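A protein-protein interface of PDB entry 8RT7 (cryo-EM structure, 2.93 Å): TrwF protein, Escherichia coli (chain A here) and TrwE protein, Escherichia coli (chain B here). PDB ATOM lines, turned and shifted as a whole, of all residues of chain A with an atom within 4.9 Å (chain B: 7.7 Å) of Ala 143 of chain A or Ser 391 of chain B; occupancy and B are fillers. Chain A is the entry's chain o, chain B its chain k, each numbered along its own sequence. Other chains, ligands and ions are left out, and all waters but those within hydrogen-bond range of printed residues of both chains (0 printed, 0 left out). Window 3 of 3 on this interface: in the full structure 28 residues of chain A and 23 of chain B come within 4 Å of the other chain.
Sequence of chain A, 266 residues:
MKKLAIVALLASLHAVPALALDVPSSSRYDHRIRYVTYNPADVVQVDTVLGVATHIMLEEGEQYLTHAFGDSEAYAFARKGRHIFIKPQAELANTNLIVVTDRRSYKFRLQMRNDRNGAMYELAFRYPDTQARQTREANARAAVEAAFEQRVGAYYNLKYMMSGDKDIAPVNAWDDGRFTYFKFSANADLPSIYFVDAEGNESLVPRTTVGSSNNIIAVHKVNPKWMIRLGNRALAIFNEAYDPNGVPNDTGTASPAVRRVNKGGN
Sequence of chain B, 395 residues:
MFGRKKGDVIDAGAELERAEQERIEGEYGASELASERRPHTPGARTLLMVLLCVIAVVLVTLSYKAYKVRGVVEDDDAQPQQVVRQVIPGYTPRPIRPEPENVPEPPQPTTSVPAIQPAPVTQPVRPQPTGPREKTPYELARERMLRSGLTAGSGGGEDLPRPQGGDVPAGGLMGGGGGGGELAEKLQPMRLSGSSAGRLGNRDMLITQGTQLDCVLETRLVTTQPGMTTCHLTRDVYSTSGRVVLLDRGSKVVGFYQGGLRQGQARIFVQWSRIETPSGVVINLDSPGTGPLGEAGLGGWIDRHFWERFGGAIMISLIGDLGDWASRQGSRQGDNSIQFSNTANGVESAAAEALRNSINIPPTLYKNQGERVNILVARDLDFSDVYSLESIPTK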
ATOM      1  N   ASN A 139     -10.830 -22.083 -20.327  1.00  0.00           N
ATOM      2  CA  ASN A 139     -11.550 -23.204 -19.734  1.00  0.00           C
ATOM      3  C   ASN A 139     -12.915 -22.764 -19.231  1.00  0.00           C
ATOM      4  O   ASN A 139     -13.915 -23.466 -19.427  1.00  0.00           O
ATOM      5  CB  ASN A 139     -10.737 -23.809 -18.591  1.00  0.00           C
ATOM      6  CG  ASN A 139      -9.418 -24.377 -19.054  1.00  0.00           C
ATOM      7  OD1 ASN A 139      -9.289 -24.823 -20.193  1.00  0.00           O
ATOM      8  ND2 ASN A 139      -8.425 -24.362 -18.173  1.00  0.00           N
ATOM      9  N   ALA A 140     -12.973 -21.600 -18.582  1.00  0.00           N
ATOM     10  CA  ALA A 140     -14.249 -21.074 -18.116  1.00  0.00           C
ATOM     11  C   ALA A 140     -15.200 -20.836 -19.277  1.00  0.00           C
ATOM     12  O   ALA A 140     -16.382 -21.169 -19.189  1.00  0.00           O
ATOM     13  CB  ALA A 140     -14.029 -19.784 -17.331  1.00  0.00           C
ATOM     14  N   ARG A 141     -14.702 -20.278 -20.379  1.00  0.00           N
ATOM     15  CA  ARG A 141     -15.563 -20.014 -21.527  1.00  0.00           C
ATOM     16  C   ARG A 141     -16.117 -21.308 -22.109  1.00  0.00           C
ATOM     17  O   ARG A 141     -17.314 -21.410 -22.405  1.00  0.00           O
ATOM     18  CB  ARG A 141     -14.791 -19.227 -22.583  1.00  0.00           C
ATOM     19  CG  ARG A 141     -15.548 -19.022 -23.881  1.00  0.00           C
ATOM     20  CD  ARG A 141     -14.862 -17.997 -24.769  1.00  0.00           C
ATOM     21  NE  ARG A 141     -13.416 -18.194 -24.823  1.00  0.00           N
ATOM     22  CZ  ARG A 141     -12.528 -17.334 -24.335  1.00  0.00           C
ATOM     23  NH1 ARG A 141     -11.230 -17.595 -24.422  1.00  0.00           N
ATOM     24  NH2 ARG A 141     -12.938 -16.214 -23.755  1.00  0.00           N
ATOM     25  N   ALA A 142     -15.259 -22.317 -22.267  1.00  0.00           N
ATOM     26  CA  ALA A 142     -15.723 -23.588 -22.814  1.00  0.00           C
ATOM     27  C   ALA A 142     -16.746 -24.247 -21.895  1.00  0.00           C
ATOM     28  O   ALA A 142     -17.782 -24.745 -22.358  1.00  0.00           O
ATOM     29  CB  ALA A 142     -14.537 -24.518 -23.054  1.00  0.00           C
ATOM     30  N   ALA A 143     -16.475 -24.249 -20.587  1.00  0.00           N
ATOM     31  CA  ALA A 143     -17.396 -24.855 -19.634  1.00  0.00           C
ATOM     32  C   ALA A 143     -18.729 -24.122 -19.604  1.00  0.00           C
ATOM     33  O   ALA A 143     -19.788 -24.751 -19.526  1.00  0.00           O
ATOM     34  CB  ALA A 143     -16.766 -24.879 -18.245  1.00  0.00           C
ATOM     35  N   VAL A 144     -18.699 -22.789 -19.657  1.00  0.00           N
ATOM     36  CA  VAL A 144     -19.929 -22.000 -19.662  1.00  0.00           C
ATOM     37  C   VAL A 144     -20.754 -22.285 -20.905  1.00  0.00           C
ATOM     38  O   VAL A 144     -21.983 -22.418 -20.834  1.00  0.00           O
ATOM     39  CB  VAL A 144     -19.598 -20.504 -19.530  1.00  0.00           C
ATOM     40  CG1 VAL A 144     -20.833 -19.692 -19.655  1.00  0.00           C
ATOM     41  CG2 VAL A 144     -19.012 -20.238 -18.169  1.00  0.00           C
ATOM     42  N   GLU A 145     -20.106 -22.363 -22.065  1.00  0.00           N
ATOM     43  CA  GLU A 145     -20.858 -22.656 -23.278  1.00  0.00           C
ATOM     44  C   GLU A 145     -21.483 -24.042 -23.205  1.00  0.00           C
ATOM     45  O   GLU A 145     -22.664 -24.226 -23.539  1.00  0.00           O
ATOM     46  CB  GLU A 145     -19.947 -22.537 -24.492  1.00  0.00           C
ATOM     47  CG  GLU A 145     -20.661 -22.703 -25.801  1.00  0.00           C
ATOM     48  CD  GLU A 145     -21.624 -21.571 -26.064  1.00  0.00           C
ATOM     49  OE1 GLU A 145     -21.400 -20.468 -25.527  1.00  0.00           O
ATOM     50  OE2 GLU A 145     -22.596 -21.775 -26.817  1.00  0.00           O
ATOM     51  N   ALA A 146     -20.714 -25.029 -22.737  1.00  0.00           N
ATOM     52  CA  ALA A 146     -21.256 -26.375 -22.600  1.00  0.00           C
ATOM     53  C   ALA A 146     -22.401 -26.410 -21.599  1.00  0.00           C
ATOM     54  O   ALA A 146     -23.346 -27.185 -21.757  1.00  0.00           O
ATOM     55  CB  ALA A 146     -20.154 -27.346 -22.185  1.00  0.00           C
ATOM     56  N   ALA A 147     -22.336 -25.574 -20.563  1.00  0.00           N
ATOM     57  CA  ALA A 147     -23.381 -25.587 -19.548  1.00  0.00           C
ATOM     58  C   ALA A 147     -24.654 -24.905 -20.025  1.00  0.00           C
ATOM     59  O   ALA A 147     -25.749 -25.320 -19.634  1.00  0.00           O
ATOM     60  CB  ALA A 147     -22.878 -24.936 -18.265  1.00  0.00           C
ATOM     61  N   ALA A 257     -26.772 -23.889 -14.221  1.00  0.00           N
ATOM     62  CA  ALA A 257     -25.428 -24.425 -14.339  1.00  0.00           C
ATOM     63  C   ALA A 257     -24.395 -23.370 -14.694  1.00  0.00           C
ATOM     64  O   ALA A 257     -23.229 -23.711 -14.899  1.00  0.00           O
ATOM     65  CB  ALA A 257     -25.397 -25.538 -15.383  1.00  0.00           C
ATOM     66  N   VAL A 258     -24.790 -22.106 -14.794  1.00  0.00           N
ATOM     67  CA  VAL A 258     -23.869 -21.011 -15.068  1.00  0.00           C
ATOM     68  C   VAL A 258     -24.147 -19.909 -14.061  1.00  0.00           C
ATOM     69  O   VAL A 258     -25.307 -19.632 -13.748  1.00  0.00           O
ATOM     70  CB  VAL A 258     -24.010 -20.479 -16.506  1.00  0.00           C
ATOM     71  CG1 VAL A 258     -22.953 -19.442 -16.792  1.00  0.00           C
ATOM     72  CG2 VAL A 258     -23.908 -21.598 -17.495  1.00  0.00           C
ATOM     73  N   ARG A 259     -23.090 -19.287 -13.555  1.00  0.00           N
ATOM     74  CA  ARG A 259     -23.180 -18.247 -12.544  1.00  0.00           C
ATOM     75  C   ARG A 259     -22.629 -16.938 -13.096  1.00  0.00           C
ATOM     76  O   ARG A 259     -21.609 -16.929 -13.787  1.00  0.00           O
ATOM     77  CB  ARG A 259     -22.405 -18.663 -11.295  1.00  0.00           C
ATOM     78  CG  ARG A 259     -22.203 -17.573 -10.279  1.00  0.00           C
ATOM     79  CD  ARG A 259     -22.236 -18.124  -8.877  1.00  0.00           C
ATOM     80  NE  ARG A 259     -23.598 -18.313  -8.396  1.00  0.00           N
ATOM     81  CZ  ARG A 259     -23.949 -19.240  -7.512  1.00  0.00           C
ATOM     82  NH1 ARG A 259     -25.210 -19.347  -7.125  1.00  0.00           N
ATOM     83  NH2 ARG A 259     -23.034 -20.063  -7.020  1.00  0.00           N
ATOM     84  N   LEU B 389     -18.856 -14.806 -16.540  1.00  0.00           N
ATOM     85  CA  LEU B 389     -19.610 -16.034 -16.351  1.00  0.00           C
ATOM     86  C   LEU B 389     -18.680 -17.167 -15.959  1.00  0.00           C
ATOM     87  O   LEU B 389     -17.598 -17.320 -16.528  1.00  0.00           O
ATOM     88  CB  LEU B 389     -20.369 -16.420 -17.616  1.00  0.00           C
ATOM     89  CG  LEU B 389     -21.189 -15.339 -18.306  1.00  0.00           C
ATOM     90  CD1 LEU B 389     -21.606 -15.808 -19.673  1.00  0.00           C
ATOM     91  CD2 LEU B 389     -22.389 -14.969 -17.477  1.00  0.00           C
ATOM     92  N   GLU B 390     -19.106 -17.960 -14.987  1.00  0.00           N
ATOM     93  CA  GLU B 390     -18.407 -19.175 -14.615  1.00  0.00           C
ATOM     94  C   GLU B 390     -19.414 -20.307 -14.528  1.00  0.00           C
ATOM     95  O   GLU B 390     -20.582 -20.093 -14.207  1.00  0.00           O
ATOM     96  CB  GLU B 390     -17.668 -19.020 -13.287  1.00  0.00           C
ATOM     97  CG  GLU B 390     -18.522 -19.271 -12.060  1.00  0.00           C
ATOM     98  CD  GLU B 390     -17.813 -18.912 -10.771  1.00  0.00           C
ATOM     99  OE1 GLU B 390     -16.753 -18.257 -10.836  1.00  0.00           O
ATOM    100  OE2 GLU B 390     -18.316 -19.283  -9.691  1.00  0.00           O
ATOM    101  N   SER B 391     -18.958 -21.513 -14.831  1.00  0.00           N
ATOM    102  CA  SER B 391     -19.834 -22.672 -14.805  1.00  0.00           C
ATOM    103  C   SER B 391     -19.870 -23.269 -13.407  1.00  0.00           C
ATOM    104  O   SER B 391     -18.827 -23.562 -12.820  1.00  0.00           O
ATOM    105  CB  SER B 391     -19.368 -23.717 -15.810  1.00  0.00           C
ATOM    106  OG  SER B 391     -19.903 -24.987 -15.495  1.00  0.00           O
ATOM    107  N   ILE B 392     -21.070 -23.444 -12.877  1.00  0.00           N
ATOM    108  CA  ILE B 392     -21.224 -24.089 -11.572  1.00  0.00           C
ATOM    109  C   ILE B 392     -20.845 -25.560 -11.698  1.00  0.00           C
ATOM    110  O   ILE B 392     -21.377 -26.258 -12.581  1.00  0.00           O
ATOM    111  CB  ILE B 392     -22.654 -23.936 -11.070  1.00  0.00           C
ATOM    112  CG1 ILE B 392     -22.891 -22.513 -10.572  1.00  0.00           C
ATOM    113  CG2 ILE B 392     -22.947 -24.947  -9.979  1.00  0.00           C
ATOM    114  CD1 ILE B 392     -24.263 -22.296 -10.017  1.00  0.00           C
ATOM    115  N   PRO B 393     -19.936 -26.068 -10.864  1.00  0.00           N
ATOM    116  CA  PRO B 393     -19.557 -27.481 -10.960  1.00  0.00           C
ATOM    117  C   PRO B 393     -20.772 -28.387 -10.837  1.00  0.00           C
ATOM    118  O   PRO B 393     -21.677 -28.143 -10.038  1.00  0.00           O
ATOM    119  CB  PRO B 393     -18.589 -27.682  -9.791  1.00  0.00           C
ATOM    120  CG  PRO B 393     -18.253 -26.331  -9.278  1.00  0.00           C
ATOM    121  CD  PRO B 393     -19.063 -25.294  -9.969  1.00  0.00           C
ATOM    122  N   THR B 394     -20.774 -29.442 -11.648  1.00  0.00           N
ATOM    123  CA  THR B 394     -21.946 -30.291 -11.801  1.00  0.00           C
ATOM    124  C   THR B 394     -22.284 -31.008 -10.502  1.00  0.00           C
ATOM    125  O   THR B 394     -21.402 -31.522  -9.808  1.00  0.00           O
ATOM    126  CB  THR B 394     -21.705 -31.311 -12.911  1.00  0.00           C
ATOM    127  OG1 THR B 394     -20.420 -31.917 -12.723  1.00  0.00           O
ATOM    128  CG2 THR B 394     -21.733 -30.631 -14.271  1.00  0.00           C
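The backbone carbonyl oxygen (O) of Glu 390 of chain B sits at hydrogen-bond distance from the backbone NH (N) of Arg 259 of chain A, 2.7 Å away.
The backbone NH of Ile 392 of chain B lies within hydrogen-bond range of the backbone carbonyl oxygen of Ala 257 of chain A.
CB of Ala 143 of chain A touches CB of Ser 391 of chain B (3.7 Å).
O of Leu 389 of chain B touches CG2 of Val 144 of chain A, at 3.6 Å.
Glu 390 of chain B touches Val 144 of chain A (C to CG2, 3.7 Å).
Ser 391 of chain B touches Val 144 of chain A.
CA of Ser 391 of chain B touches O of Ala 257 of chain A, at 3.6 Å.
Glu 390 of chain B touches Val 258 of chain A (O to CA, 3.5 Å).
Leu 389 of chain B touches Arg 259 of chain A.
CD1 of Ile 392 of chain B touches NH2 of Arg 259 of chain A, at 3.9 Å.
Ala 143 of chain A touches just one residue of chain B: Ser 391.
Of chain A, only Ala 143 (3.7 Å), Val 144 (3.6 Å) and Ala 257 (3.6 Å) come within 4 Å of Ser 391 of chain B.
No residue of chain B comes within 4 Å of Ala 142 of chain A.
Of the printed residues of chain B, Val 258 of chain A touches Glu 390 (3.5 Å).
Of the printed residues of chain A, Ile 392 of chain B touches Ala 257 (3.0 Å) and Arg 259 (3.9 Å).
Of the printed residues of chain B, Ala 257 of chain A touches Ser 391 and Ile 392.
Of the 12 printed residues of chain A, 5 touch a printed residue of chain B.
Printed residues of chain A that touch a printed residue of chain B: Ala 143, Val 144, Ala 257, Val 258 and Arg 259.
Hydrophobic or aromatic side chains of chain A within 4 Å of the printed part of chain B: Ala 143, Val 144 and Val 258.
Of the 6 printed residues of chain B, 4 touch a printed residue of chain A.
Printed residues of chain B that touch a printed residue of chain A: Leu 389, Glu 390, Ser 391 and Ile 392.
Hydrophobic or aromatic side chains of chain B that line the printed part of chain A: Leu 389 and Ile 392.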
